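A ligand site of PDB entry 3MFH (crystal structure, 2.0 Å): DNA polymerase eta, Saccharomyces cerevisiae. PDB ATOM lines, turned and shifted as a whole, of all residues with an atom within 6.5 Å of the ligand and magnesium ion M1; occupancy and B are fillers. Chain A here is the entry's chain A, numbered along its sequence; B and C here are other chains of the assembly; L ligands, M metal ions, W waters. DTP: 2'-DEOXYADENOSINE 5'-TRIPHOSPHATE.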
ATOM      1  N   ASP A  37     -10.849  18.539   5.130  1.00  0.00           N
ATOM      2  CA  ASP A  37     -11.664  19.167   6.141  1.00  0.00           C
ATOM      3  C   ASP A  37     -11.187  18.721   7.534  1.00  0.00           C
ATOM      4  O   ASP A  37     -11.101  17.536   7.808  1.00  0.00           O
ATOM      5  CB  ASP A  37     -13.100  18.771   5.925  1.00  0.00           C
ATOM      6  CG  ASP A  37     -14.051  19.461   6.859  1.00  0.00           C
ATOM      7  OD1 ASP A  37     -13.968  19.226   8.074  1.00  0.00           O
ATOM      8  OD2 ASP A  37     -14.918  20.230   6.384  1.00  0.00           O
ATOM      9  N   MET A  38     -10.899  19.685   8.393  1.00  0.00           N
ATOM     10  CA  MET A  38     -10.385  19.424   9.736  1.00  0.00           C
ATOM     11  C   MET A  38     -11.453  18.731  10.563  1.00  0.00           C
ATOM     12  O   MET A  38     -12.608  19.128  10.547  1.00  0.00           O
ATOM     13  CB  MET A  38     -10.012  20.732  10.419  1.00  0.00           C
ATOM     14  CG  MET A  38      -8.946  21.516   9.698  1.00  0.00           C
ATOM     15  SD  MET A  38      -7.345  20.825  10.114  1.00  0.00           S
ATOM     16  CE  MET A  38      -6.295  21.808   9.059  1.00  0.00           C
ATOM     17  N   ASN A  39     -11.059  17.668  11.258  1.00  0.00           N
ATOM     18  CA  ASN A  39     -11.981  16.903  12.077  1.00  0.00           C
ATOM     19  C   ASN A  39     -12.318  17.734  13.339  1.00  0.00           C
ATOM     20  O   ASN A  39     -11.413  18.242  13.990  1.00  0.00           O
ATOM     21  CB  ASN A  39     -11.332  15.554  12.508  1.00  0.00           C
ATOM     22  CG  ASN A  39     -11.132  14.572  11.355  1.00  0.00           C
ATOM     23  OD1 ASN A  39     -10.185  13.780  11.385  1.00  0.00           O
ATOM     24  ND2 ASN A  39     -12.019  14.589  10.355  1.00  0.00           N
ATOM     25  N   ALA A  40     -13.610  17.873  13.657  1.00  0.00           N
ATOM     26  CA  ALA A  40     -14.052  18.468  14.914  1.00  0.00           C
ATOM     27  C   ALA A  40     -13.246  19.732  15.223  1.00  0.00           C
ATOM     28  O   ALA A  40     -12.689  19.881  16.306  1.00  0.00           O
ATOM     29  CB  ALA A  40     -13.900  17.419  16.088  1.00  0.00           C
ATOM     30  N   PHE A  41     -13.178  20.644  14.271  1.00  0.00           N
ATOM     31  CA  PHE A  41     -12.128  21.654  14.298  1.00  0.00           C
ATOM     32  C   PHE A  41     -12.008  22.456  15.609  1.00  0.00           C
ATOM     33  O   PHE A  41     -10.960  22.449  16.211  1.00  0.00           O
ATOM     34  CB  PHE A  41     -12.232  22.575  13.089  1.00  0.00           C
ATOM     35  CG  PHE A  41     -11.116  23.544  12.983  1.00  0.00           C
ATOM     36  CD1 PHE A  41      -9.783  23.127  13.106  1.00  0.00           C
ATOM     37  CD2 PHE A  41     -11.364  24.890  12.761  1.00  0.00           C
ATOM     38  CE1 PHE A  41      -8.729  24.070  13.025  1.00  0.00           C
ATOM     39  CE2 PHE A  41     -10.331  25.805  12.670  1.00  0.00           C
ATOM     40  CZ  PHE A  41      -9.015  25.391  12.808  1.00  0.00           C
ATOM     41  N   PHE A  42     -13.051  23.157  16.049  1.00  0.00           N
ATOM     42  CA  PHE A  42     -12.902  24.025  17.214  1.00  0.00           C
ATOM     43  C   PHE A  42     -12.560  23.185  18.448  1.00  0.00           C
ATOM     44  O   PHE A  42     -11.858  23.661  19.324  1.00  0.00           O
ATOM     45  CB  PHE A  42     -14.144  24.852  17.494  1.00  0.00           C
ATOM     46  CG  PHE A  42     -14.430  25.938  16.480  1.00  0.00           C
ATOM     47  CD1 PHE A  42     -13.743  26.024  15.270  1.00  0.00           C
ATOM     48  CD2 PHE A  42     -15.442  26.847  16.720  1.00  0.00           C
ATOM     49  CE1 PHE A  42     -14.040  26.994  14.347  1.00  0.00           C
ATOM     50  CE2 PHE A  42     -15.745  27.838  15.799  1.00  0.00           C
ATOM     51  CZ  PHE A  42     -15.048  27.893  14.605  1.00  0.00           C
ATOM     52  N   ALA A  43     -13.049  21.948  18.504  1.00  0.00           N
ATOM     53  CA  ALA A  43     -12.776  21.064  19.648  1.00  0.00           C
ATOM     54  C   ALA A  43     -11.328  20.615  19.643  1.00  0.00           C
ATOM     55  O   ALA A  43     -10.704  20.564  20.679  1.00  0.00           O
ATOM     56  CB  ALA A  43     -13.685  19.867  19.657  1.00  0.00           C
ATOM     57  N   GLN A  62     -20.316  27.556  22.945  1.00  0.00           N
ATOM     58  CA  GLN A  62     -20.574  28.949  22.657  1.00  0.00           C
ATOM     59  C   GLN A  62     -21.905  29.300  23.300  1.00  0.00           C
ATOM     60  O   GLN A  62     -22.977  28.944  22.784  1.00  0.00           O
ATOM     61  CB  GLN A  62     -20.624  29.215  21.148  1.00  0.00           C
ATOM     62  CG  GLN A  62     -20.703  30.679  20.774  1.00  0.00           C
ATOM     63  CD  GLN A  62     -20.720  30.907  19.274  1.00  0.00           C
ATOM     64  OE1 GLN A  62     -19.674  31.217  18.677  1.00  0.00           O
ATOM     65  NE2 GLN A  62     -21.898  30.728  18.657  1.00  0.00           N
ATOM     66  N   ILE A  67     -20.720  23.910  19.945  1.00  0.00           N
ATOM     67  CA  ILE A  67     -20.400  24.404  18.593  1.00  0.00           C
ATOM     68  C   ILE A  67     -19.502  23.395  17.877  1.00  0.00           C
ATOM     69  O   ILE A  67     -19.491  23.327  16.637  1.00  0.00           O
ATOM     70  CB  ILE A  67     -19.816  25.855  18.650  1.00  0.00           C
ATOM     71  CG1 ILE A  67     -19.687  26.486  17.291  1.00  0.00           C
ATOM     72  CG2 ILE A  67     -18.426  25.902  19.287  1.00  0.00           C
ATOM     73  CD1 ILE A  67     -19.365  27.993  17.360  1.00  0.00           C
ATOM     74  N   ALA A  68     -18.763  22.598  18.657  1.00  0.00           N
ATOM     75  CA  ALA A  68     -17.979  21.486  18.111  1.00  0.00           C
ATOM     76  C   ALA A  68     -17.822  20.349  19.109  1.00  0.00           C
ATOM     77  O   ALA A  68     -17.665  20.559  20.322  1.00  0.00           O
ATOM     78  CB  ALA A  68     -16.594  21.984  17.620  1.00  0.00           C
ATOM     79  N   VAL A  69     -17.871  19.123  18.602  1.00  0.00           N
ATOM     80  CA  VAL A  69     -17.797  17.940  19.450  1.00  0.00           C
ATOM     81  C   VAL A  69     -16.658  17.071  18.968  1.00  0.00           C
ATOM     82  O   VAL A  69     -16.710  16.540  17.853  1.00  0.00           O
ATOM     83  CB  VAL A  69     -19.147  17.157  19.454  1.00  0.00           C
ATOM     84  CG1 VAL A  69     -19.653  16.969  18.083  1.00  0.00           C
ATOM     85  CG2 VAL A  69     -19.015  15.785  20.170  1.00  0.00           C
ATOM     86  N   TYR A  71     -14.244  13.813  18.571  1.00  0.00           N
ATOM     87  CA  TYR A  71     -14.598  12.425  18.254  1.00  0.00           C
ATOM     88  C   TYR A  71     -14.669  11.529  19.497  1.00  0.00           C
ATOM     89  O   TYR A  71     -15.480  10.583  19.526  1.00  0.00           O
ATOM     90  CB  TYR A  71     -13.717  11.851  17.143  1.00  0.00           C
ATOM     91  CG  TYR A  71     -14.210  12.377  15.791  1.00  0.00           C
ATOM     92  CD1 TYR A  71     -13.892  13.659  15.367  1.00  0.00           C
ATOM     93  CD2 TYR A  71     -15.089  11.642  15.015  1.00  0.00           C
ATOM     94  CE1 TYR A  71     -14.355  14.165  14.162  1.00  0.00           C
ATOM     95  CE2 TYR A  71     -15.552  12.130  13.800  1.00  0.00           C
ATOM     96  CZ  TYR A  71     -15.186  13.397  13.385  1.00  0.00           C
ATOM     97  OH  TYR A  71     -15.667  13.899  12.207  1.00  0.00           O
ATOM     98  N   ARG A  74     -18.209  12.175  20.709  1.00  0.00           N
ATOM     99  CA  ARG A  74     -19.230  11.597  19.824  1.00  0.00           C
ATOM    100  C   ARG A  74     -19.529  10.117  20.130  1.00  0.00           C
ATOM    101  O   ARG A  74     -20.628   9.611  19.813  1.00  0.00           O
ATOM    102  CB  ARG A  74     -18.834  11.746  18.358  1.00  0.00           C
ATOM    103  CG  ARG A  74     -18.658  13.197  17.888  1.00  0.00           C
ATOM    104  CD  ARG A  74     -18.328  13.278  16.398  1.00  0.00           C
ATOM    105  NE  ARG A  74     -17.795  14.601  16.096  1.00  0.00           N
ATOM    106  CZ  ARG A  74     -17.835  15.191  14.915  1.00  0.00           C
ATOM    107  NH1 ARG A  74     -18.417  14.593  13.888  1.00  0.00           N
ATOM    108  NH2 ARG A  74     -17.337  16.426  14.778  1.00  0.00           N
ATOM    109  N   ARG A  80     -23.367  18.083  17.616  1.00  0.00           N
ATOM    110  CA  ARG A  80     -23.274  19.538  17.499  1.00  0.00           C
ATOM    111  C   ARG A  80     -24.664  20.077  17.699  1.00  0.00           C
ATOM    112  O   ARG A  80     -25.646  19.486  17.267  1.00  0.00           O
ATOM    113  CB  ARG A  80     -22.752  19.974  16.116  1.00  0.00           C
ATOM    114  CG  ARG A  80     -21.557  20.922  16.157  1.00  0.00           C
ATOM    115  CD  ARG A  80     -21.056  21.266  14.731  1.00  0.00           C
ATOM    116  NE  ARG A  80     -22.134  21.918  14.022  1.00  0.00           N
ATOM    117  CZ  ARG A  80     -22.524  23.168  14.235  1.00  0.00           C
ATOM    118  NH1 ARG A  80     -21.888  23.968  15.095  1.00  0.00           N
ATOM    119  NH2 ARG A  80     -23.574  23.632  13.560  1.00  0.00           N
ATOM    120  N   MET A  81     -24.729  21.209  18.379  1.00  0.00           N
ATOM    121  CA  MET A  81     -25.977  21.928  18.650  1.00  0.00           C
ATOM    122  C   MET A  81     -26.847  21.295  19.734  1.00  0.00           C
ATOM    123  O   MET A  81     -27.925  21.834  20.049  1.00  0.00           O
ATOM    124  CB  MET A  81     -26.761  22.254  17.369  1.00  0.00           C
ATOM    125  CG  MET A  81     -26.195  23.447  16.607  1.00  0.00           C
ATOM    126  SD  MET A  81     -26.147  24.898  17.694  1.00  0.00           S
ATOM    127  CE  MET A  81     -27.888  25.334  17.799  1.00  0.00           C
ATOM    128  N   LEU A 135     -13.641  34.289  17.894  1.00  0.00           N
ATOM    129  CA  LEU A 135     -13.280  33.099  17.118  1.00  0.00           C
ATOM    130  C   LEU A 135     -11.825  33.144  16.672  1.00  0.00           C
ATOM    131  O   LEU A 135     -11.381  32.266  15.929  1.00  0.00           O
ATOM    132  CB  LEU A 135     -14.190  32.958  15.901  1.00  0.00           C
ATOM    133  CG  LEU A 135     -15.689  32.849  16.167  1.00  0.00           C
ATOM    134  CD1 LEU A 135     -16.422  32.696  14.851  1.00  0.00           C
ATOM    135  CD2 LEU A 135     -16.010  31.682  17.145  1.00  0.00           C
ATOM    136  N   SER A 160     -13.434  27.545   3.597  1.00  0.00           N
ATOM    137  CA  SER A 160     -14.078  28.027   4.826  1.00  0.00           C
ATOM    138  C   SER A 160     -13.057  27.859   5.945  1.00  0.00           C
ATOM    139  O   SER A 160     -11.914  27.483   5.686  1.00  0.00           O
ATOM    140  CB  SER A 160     -15.394  27.270   5.125  1.00  0.00           C
ATOM    141  OG  SER A 160     -15.155  25.918   5.464  1.00  0.00           O
ATOM    142  N   ILE A 161     -13.431  28.186   7.175  1.00  0.00           N
ATOM    143  CA  ILE A 161     -12.445  28.218   8.257  1.00  0.00           C
ATOM    144  C   ILE A 161     -11.662  26.884   8.386  1.00  0.00           C
ATOM    145  O   ILE A 161     -10.476  26.900   8.715  1.00  0.00           O
ATOM    146  CB  ILE A 161     -13.037  28.628   9.601  1.00  0.00           C
ATOM    147  CG1 ILE A 161     -11.894  29.001  10.558  1.00  0.00           C
ATOM    148  CG2 ILE A 161     -13.960  27.503  10.181  1.00  0.00           C
ATOM    149  CD1 ILE A 161     -12.307  29.901  11.666  1.00  0.00           C
ATOM    150  N   ASP A 162     -12.277  25.764   8.046  1.00  0.00           N
ATOM    151  CA  ASP A 162     -11.591  24.480   8.227  1.00  0.00           C
ATOM    152  C   ASP A 162     -11.511  23.575   6.989  1.00  0.00           C
ATOM    153  O   ASP A 162     -11.141  22.388   7.106  1.00  0.00           O
ATOM    154  CB  ASP A 162     -12.180  23.751   9.459  1.00  0.00           C
ATOM    155  CG  ASP A 162     -13.259  22.761   9.114  1.00  0.00           C
ATOM    156  OD1 ASP A 162     -13.316  21.736   9.830  1.00  0.00           O
ATOM    157  OD2 ASP A 162     -14.087  22.971   8.178  1.00  0.00           O
ATOM    158  N   GLU A 163     -11.827  24.138   5.830  1.00  0.00           N
ATOM    159  CA  GLU A 163     -11.796  23.424   4.550  1.00  0.00           C
ATOM    160  C   GLU A 163     -10.800  24.066   3.604  1.00  0.00           C
ATOM    161  O   GLU A 163     -10.750  25.305   3.510  1.00  0.00           O
ATOM    162  CB  GLU A 163     -13.130  23.515   3.824  1.00  0.00           C
ATOM    163  CG  GLU A 163     -14.339  22.926   4.514  1.00  0.00           C
ATOM    164  CD  GLU A 163     -15.585  23.164   3.662  1.00  0.00           C
ATOM    165  OE1 GLU A 163     -16.587  23.591   4.278  1.00  0.00           O
ATOM    166  OE2 GLU A 163     -15.556  22.981   2.405  1.00  0.00           O
ATOM    167  N   SER A 268     -10.218  14.709   7.490  1.00  0.00           N
ATOM    168  CA  SER A 268     -10.802  13.809   6.521  1.00  0.00           C
ATOM    169  C   SER A 268     -10.616  14.453   5.162  1.00  0.00           C
ATOM    170  O   SER A 268     -10.527  15.681   5.045  1.00  0.00           O
ATOM    171  CB  SER A 268     -12.264  13.593   6.841  1.00  0.00           C
ATOM    172  OG  SER A 268     -12.328  12.668   7.924  1.00  0.00           O
ATOM    173  N   ASN A 283     -16.448  14.054   3.467  1.00  0.00           N
ATOM    174  CA  ASN A 283     -17.441  13.892   4.531  1.00  0.00           C
ATOM    175  C   ASN A 283     -17.923  12.442   4.669  1.00  0.00           C
ATOM    176  O   ASN A 283     -18.685  12.126   5.543  1.00  0.00           O
ATOM    177  CB  ASN A 283     -18.626  14.824   4.253  1.00  0.00           C
ATOM    178  CG  ASN A 283     -19.326  15.294   5.523  1.00  0.00           C
ATOM    179  OD1 ASN A 283     -18.691  15.793   6.481  1.00  0.00           O
ATOM    180  ND2 ASN A 283     -20.635  15.156   5.529  1.00  0.00           N
ATOM    181  N   LYS A 286     -15.123   9.726   8.627  1.00  0.00           N
ATOM    182  CA  LYS A 286     -14.438  10.542   9.609  1.00  0.00           C
ATOM    183  C   LYS A 286     -14.334   9.763  10.934  1.00  0.00           C
ATOM    184  O   LYS A 286     -15.209   8.949  11.226  1.00  0.00           O
ATOM    185  CB  LYS A 286     -15.258  11.797   9.949  1.00  0.00           C
ATOM    186  CG  LYS A 286     -15.986  12.578   8.856  1.00  0.00           C
ATOM    187  CD  LYS A 286     -17.284  13.162   9.508  1.00  0.00           C
ATOM    188  CE  LYS A 286     -17.847  14.230   8.691  1.00  0.00           C
ATOM    189  NZ  LYS A 286     -18.871  14.992   9.400  1.00  0.00           N
ATOM    190  N   PRO A 287     -13.313  10.057  11.757  1.00  0.00           N
ATOM    191  CA  PRO A 287     -12.216  11.015  11.521  1.00  0.00           C
ATOM    192  C   PRO A 287     -11.027  10.358  10.854  1.00  0.00           C
ATOM    193  O   PRO A 287     -11.020   9.151  10.633  1.00  0.00           O
ATOM    194  CB  PRO A 287     -11.804  11.405  12.935  1.00  0.00           C
ATOM    195  CG  PRO A 287     -11.928  10.069  13.702  1.00  0.00           C
ATOM    196  CD  PRO A 287     -13.114   9.331  13.029  1.00  0.00           C
ATOM    197  O5'  DT B   4     -32.399  28.302  16.498  1.00  0.00           O
ATOM    198  C5'  DT B   4     -31.013  27.935  16.615  1.00  0.00           C
ATOM    199  C4'  DT B   4     -30.227  28.908  17.494  1.00  0.00           C
ATOM    200  O4'  DT B   4     -28.882  28.393  17.696  1.00  0.00           O
ATOM    201  C3'  DT B   4     -30.028  30.332  16.949  1.00  0.00           C
ATOM    202  O3'  DT B   4     -29.973  31.241  18.032  1.00  0.00           O
ATOM    203  C2'  DT B   4     -28.694  30.212  16.211  1.00  0.00           C
ATOM    204  C1'  DT B   4     -27.919  29.264  17.150  1.00  0.00           C
ATOM    205  N1   DT B   4     -26.836  28.400  16.550  1.00  0.00           N
ATOM    206  C2   DT B   4     -27.079  27.681  15.400  1.00  0.00           C
ATOM    207  O2   DT B   4     -28.140  27.713  14.793  1.00  0.00           O
ATOM    208  N3   DT B   4     -26.028  26.898  14.967  1.00  0.00           N
ATOM    209  C4   DT B   4     -24.776  26.771  15.546  1.00  0.00           C
ATOM    210  O4   DT B   4     -23.923  26.033  15.064  1.00  0.00           O
ATOM    211  C5   DT B   4     -24.576  27.540  16.772  1.00  0.00           C
ATOM    212  C7   DT B   4     -23.254  27.474  17.492  1.00  0.00           C
ATOM    213  C6   DT B   4     -25.601  28.297  17.211  1.00  0.00           C
ATOM    214  P    DT B   5     -29.585  32.787  17.881  1.00  0.00           P
ATOM    215  OP1  DT B   5     -30.007  33.387  19.152  1.00  0.00           O
ATOM    216  OP2  DT B   5     -30.027  33.291  16.573  1.00  0.00           O
ATOM    217  O5'  DT B   5     -27.960  32.823  17.822  1.00  0.00           O
ATOM    218  C5'  DT B   5     -27.209  32.583  19.005  1.00  0.00           C
ATOM    219  C4'  DT B   5     -25.732  32.645  18.719  1.00  0.00           C
ATOM    220  O4'  DT B   5     -25.379  31.712  17.672  1.00  0.00           O
ATOM    221  C3'  DT B   5     -25.230  34.015  18.242  1.00  0.00           C
ATOM    222  O3'  DT B   5     -24.052  34.275  18.942  1.00  0.00           O
ATOM    223  C2'  DT B   5     -25.054  33.823  16.728  1.00  0.00           C
ATOM    224  C1'  DT B   5     -24.573  32.369  16.712  1.00  0.00           C
ATOM    225  N1   DT B   5     -24.758  31.514  15.499  1.00  0.00           N
ATOM    226  C2   DT B   5     -23.780  30.590  15.181  1.00  0.00           C
ATOM    227  O2   DT B   5     -22.746  30.482  15.801  1.00  0.00           O
ATOM    228  N3   DT B   5     -24.072  29.796  14.105  1.00  0.00           N
ATOM    229  C4   DT B   5     -25.232  29.835  13.332  1.00  0.00           C
ATOM    230  O4   DT B   5     -25.418  29.088  12.387  1.00  0.00           O
ATOM    231  C5   DT B   5     -26.231  30.803  13.718  1.00  0.00           C
ATOM    232  C7   DT B   5     -27.514  30.915  12.932  1.00  0.00           C
ATOM    233  C6   DT B   5     -25.944  31.591  14.782  1.00  0.00           C
ATOM    234  P    DG B   6     -23.294  35.670  18.852  1.00  0.00           P
ATOM    235  OP1  DG B   6     -22.554  35.825  20.122  1.00  0.00           O
ATOM    236  OP2  DG B   6     -24.222  36.709  18.357  1.00  0.00           O
ATOM    237  O5'  DG B   6     -22.235  35.409  17.711  1.00  0.00           O
ATOM    238  C5'  DG B   6     -21.068  34.611  18.016  1.00  0.00           C
ATOM    239  C4'  DG B   6     -20.275  34.393  16.742  1.00  0.00           C
ATOM    240  O4'  DG B   6     -21.093  33.576  15.844  1.00  0.00           O
ATOM    241  C3'  DG B   6     -19.941  35.691  15.990  1.00  0.00           C
ATOM    242  O3'  DG B   6     -18.594  35.672  15.574  1.00  0.00           O
ATOM    243  C2'  DG B   6     -20.927  35.629  14.835  1.00  0.00           C
ATOM    244  C1'  DG B   6     -20.980  34.136  14.575  1.00  0.00           C
ATOM    245  N9   DG B   6     -22.071  33.724  13.694  1.00  0.00           N
ATOM    246  C8   DG B   6     -23.298  34.321  13.490  1.00  0.00           C
ATOM    247  N7   DG B   6     -24.016  33.736  12.586  1.00  0.00           N
ATOM    248  C5   DG B   6     -23.202  32.694  12.163  1.00  0.00           C
ATOM    249  C6   DG B   6     -23.424  31.697  11.176  1.00  0.00           C
ATOM    250  O6   DG B   6     -24.426  31.567  10.492  1.00  0.00           O
ATOM    251  N1   DG B   6     -22.338  30.819  11.030  1.00  0.00           N
ATOM    252  C2   DG B   6     -21.167  30.899  11.771  1.00  0.00           C
ATOM    253  N2   DG B   6     -20.208  29.983  11.543  1.00  0.00           N
ATOM    254  N3   DG B   6     -20.962  31.828  12.694  1.00  0.00           N
ATOM    255  C4   DG B   6     -22.006  32.677  12.832  1.00  0.00           C
ATOM    256  N1  DOC C  11     -21.505  26.845   8.152  1.00  0.00           N
ATOM    257  C2  DOC C  11     -21.413  27.965   8.989  1.00  0.00           C
ATOM    258  N3  DOC C  11     -22.465  28.785   9.118  1.00  0.00           N
ATOM    259  C4  DOC C  11     -23.609  28.529   8.433  1.00  0.00           C
ATOM    260  C5  DOC C  11     -23.709  27.415   7.606  1.00  0.00           C
ATOM    261  C6  DOC C  11     -22.613  26.590   7.466  1.00  0.00           C
ATOM    262  O2  DOC C  11     -20.340  28.189   9.605  1.00  0.00           O
ATOM    263  N4  DOC C  11     -24.669  29.337   8.563  1.00  0.00           N
ATOM    264  C1' DOC C  11     -20.315  26.003   8.050  1.00  0.00           C
ATOM    265  C2' DOC C  11     -20.653  24.520   8.275  1.00  0.00           C
ATOM    266  C3' DOC C  11     -19.601  23.845   7.446  1.00  0.00           C
ATOM    267  C4' DOC C  11     -19.231  24.864   6.365  1.00  0.00           C
ATOM    268  O4' DOC C  11     -19.734  26.147   6.748  1.00  0.00           O
ATOM    269  C5' DOC C  11     -19.783  24.426   5.016  1.00  0.00           C
ATOM    270  O5' DOC C  11     -21.150  23.974   5.121  1.00  0.00           O
ATOM    271  P   DOC C  11     -21.827  23.375   3.795  1.00  0.00           P
ATOM    272  OP1 DOC C  11     -20.949  22.271   3.301  1.00  0.00           O
ATOM    273  OP2 DOC C  11     -23.257  23.061   4.109  1.00  0.00           O
HETATM  274  PG  DTP L   1     -16.230  17.369  11.235  1.00  0.00           P
HETATM  275  O1G DTP L   1     -15.699  18.149  10.078  1.00  0.00           O
HETATM  276  O2G DTP L   1     -17.542  16.646  11.084  1.00  0.00           O
HETATM  277  O3G DTP L   1     -15.190  16.466  11.862  1.00  0.00           O
HETATM  278  PB  DTP L   1     -16.306  19.998  12.444  1.00  0.00           P
HETATM  279  O1B DTP L   1     -14.950  20.281  11.866  1.00  0.00           O
HETATM  280  O2B DTP L   1     -16.539  20.379  13.919  1.00  0.00           O
HETATM  281  O3B DTP L   1     -16.645  18.434  12.374  1.00  0.00           O
HETATM  282  PA  DTP L   1     -17.454  21.499  10.234  1.00  0.00           P
HETATM  283  O1A DTP L   1     -16.327  20.969   9.389  1.00  0.00           O
HETATM  284  O2A DTP L   1     -18.837  21.520   9.682  1.00  0.00           O
HETATM  285  O3A DTP L   1     -17.534  20.650  11.622  1.00  0.00           O
HETATM  286  O5' DTP L   1     -17.118  23.008  10.686  1.00  0.00           O
HETATM  287  C5' DTP L   1     -15.831  23.428  11.109  1.00  0.00           C
HETATM  288  C4' DTP L   1     -15.932  24.272  12.375  1.00  0.00           C
HETATM  289  O4' DTP L   1     -16.741  25.421  12.103  1.00  0.00           O
HETATM  290  C3' DTP L   1     -16.578  23.571  13.573  1.00  0.00           C
HETATM  291  O3' DTP L   1     -15.608  22.869  14.375  1.00  0.00           O
HETATM  292  C2' DTP L   1     -17.270  24.684  14.336  1.00  0.00           C
HETATM  293  C1' DTP L   1     -17.584  25.673  13.226  1.00  0.00           C
HETATM  294  N9  DTP L   1     -18.998  25.617  12.774  1.00  0.00           N
HETATM  295  C8  DTP L   1     -19.593  24.691  11.983  1.00  0.00           C
HETATM  296  N7  DTP L   1     -20.916  24.978  11.785  1.00  0.00           N
HETATM  297  C5  DTP L   1     -21.173  26.093  12.449  1.00  0.00           C
HETATM  298  C6  DTP L   1     -22.361  26.939  12.651  1.00  0.00           C
HETATM  299  N6  DTP L   1     -23.545  26.613  12.076  1.00  0.00           N
HETATM  300  N1  DTP L   1     -22.209  28.025  13.448  1.00  0.00           N
HETATM  301  C2  DTP L   1     -21.032  28.331  14.019  1.00  0.00           C
HETATM  302  N3  DTP L   1     -19.924  27.609  13.878  1.00  0.00           N
HETATM  303  C4  DTP L   1     -19.932  26.505  13.120  1.00  0.00           C
HETATM  304 MG    MG M   1     -14.548  19.915   9.876  1.00  0.00          MG
HETATM  305 MG    MG M   2     -16.916  22.447   6.836  1.00  0.00          MG
HETATM  306  O   HOH W   1     -18.958  20.265   7.239  1.00  0.00           O
HETATM  307  O   HOH W   2     -17.565  27.605  10.154  1.00  0.00           O
HETATM  308  O   HOH W   3     -13.904  16.394   8.981  1.00  0.00           O
HETATM  309  O   HOH W   4     -18.086  29.911  13.991  1.00  0.00           O
HETATM  310  O   HOH W   5     -20.970  19.764  10.944  1.00  0.00           O
HETATM  311  O   HOH W   6     -26.388  25.417  12.665  1.00  0.00           O
HETATM  312  O   HOH W   7     -19.855  17.213  11.951  1.00  0.00           O
HETATM  313  O   HOH W   8     -17.198  17.989   7.745  1.00  0.00           O
HETATM  314  O   HOH W   9     -18.172  19.091  15.746  1.00  0.00           O
HETATM  315  O   HOH W  10     -24.893  24.376  10.402  1.00  0.00           O
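O3G of the ligand sits at hydrogen-bond distance from OH of Tyr 71 (2.6 Å). O4 of DT 5 of chain B is in hydrogen-bond range of N6 of the ligand, at 3.1 Å. An oxygen (O2G) of the ligand lies within salt-bridge range of the side-chain amino group of Lys 286, at 2.7 Å. The backbone NH of Ala 40 sits at hydrogen-bond distance from an oxygen (O3G) of the ligand (2.8 Å). An oxygen (O3') of the ligand sits at hydrogen-bond distance from the backbone NH (N) of Phe 41. O4 of DT 4 of chain B lies close to N6 of the ligand. The backbone NH (N) of Phe 42 sits at hydrogen-bond distance from an oxygen (O3') of the ligand (3.1 Å). NH1 of Arg 74 lies within salt-bridge range of O2G of the ligand, 3.6 Å away. N7 of the ligand sits close to NH2 of Arg 80 (3.5 Å).
Water W3 lies within hydrogen-bond range of ND2 of Asn 39 (2.9 Å), O3G of the ligand (3.2 Å) and O of Asp 37 (3.2 Å). Water W9 lies within hydrogen-bond range of an oxygen (O2B) of the ligand (2.8 Å), the backbone NH of Val 69 (2.9 Å) and the guanidinium group of Arg 74 (3.0 Å). Water W8 lies within hydrogen-bond range of the side-chain amide oxygen (OD1) of Asn 283 (2.9 Å) and the side-chain carboxylate (OD2) of Asp 37 (3.5 Å). Water W4 lies within hydrogen-bond range of a nitrogen (N3) of the ligand and N2 of DG 6 of chain B. Water W2 lies within hydrogen-bond range of O2 of DOC 11 of chain C (2.9 Å) and an oxygen (O4') of the ligand (3.0 Å). Water W6 lies within hydrogen-bond range of N3 of DT 4 of chain B (2.8 Å), N6 of the ligand (3.1 Å) and NH2 of Arg 80 (3.5 Å).
Magnesium ion M1 is bound by OD1 of Asp 37. Magnesium ion M1 is bound by O1B of the ligand (2.1 Å). O1G of the ligand is bound to magnesium ion M1, at 2.1 Å. O1A of the ligand is bound to magnesium ion M1, 2.1 Å away. Magnesium ion M1 is bound by O of Met 38, 2.2 Å away. OD1 of Asp 162 binds magnesium ion M1, at 2.2 Å.
N2 of DG 6 of chain B sits close to N3 of the ligand. Asn 39 touches the ligand (CA to O3G, 3.2 Å). Ile 67 touches the ligand. Ala 68 touches the ligand. Ile 161 touches the ligand (CG2 to O4', 3.97 Å). C3' of DOC 11 of chain C touches O2A of the ligand, 3.3 Å away. Hydrophobic or aromatic side chains within 4 Å of the ligand: Phe 41, Phe 42, Ile 67, Ala 68, Tyr 71 and Ile 161. Within 4 Å of the ligand: Asp 37, Met 38, Asn 39, Ala 40, Phe 41, Phe 42, Ile 67, Ala 68, Tyr 71, Arg 74, Arg 80, Ile 161, Asp 162, Lys 286, DT 4 of chain B, DT 5 of chain B, DG 6 of chain B and DOC 11 of chain C.
The backbone NH (N) of Asp 37 lies within hydrogen-bond range of the backbone carbonyl oxygen (O) of Ser 268. O2 of DT 5 of chain B lies within hydrogen-bond range of the side-chain amide nitrogen (NE2) of Gln 62, at 3.0 Å. The side-chain amino group (NZ) of Lys 286 sits close to the side-chain amide oxygen (OD1) of Asn 283 (3.0 Å). O4 of DT 4 of chain B is in hydrogen-bond range of the guanidinium group (NH2) of Arg 80, at 2.9 Å. O2 of DOC 11 of chain C sits close to N2 of DG 6 of chain B, 2.6 Å away. The guanidinium group (NE) of Arg 74 is in hydrogen-bond range of the backbone carbonyl oxygen (O) of Val 69, at 2.8 Å. ND2 of Asn 39 sits at hydrogen-bond distance from OG of Ser 268 (3.1 Å). The guanidinium group (NH1) of Arg 80 sits at hydrogen-bond distance from the backbone carbonyl oxygen (O) of Ile 67 (2.9 Å).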
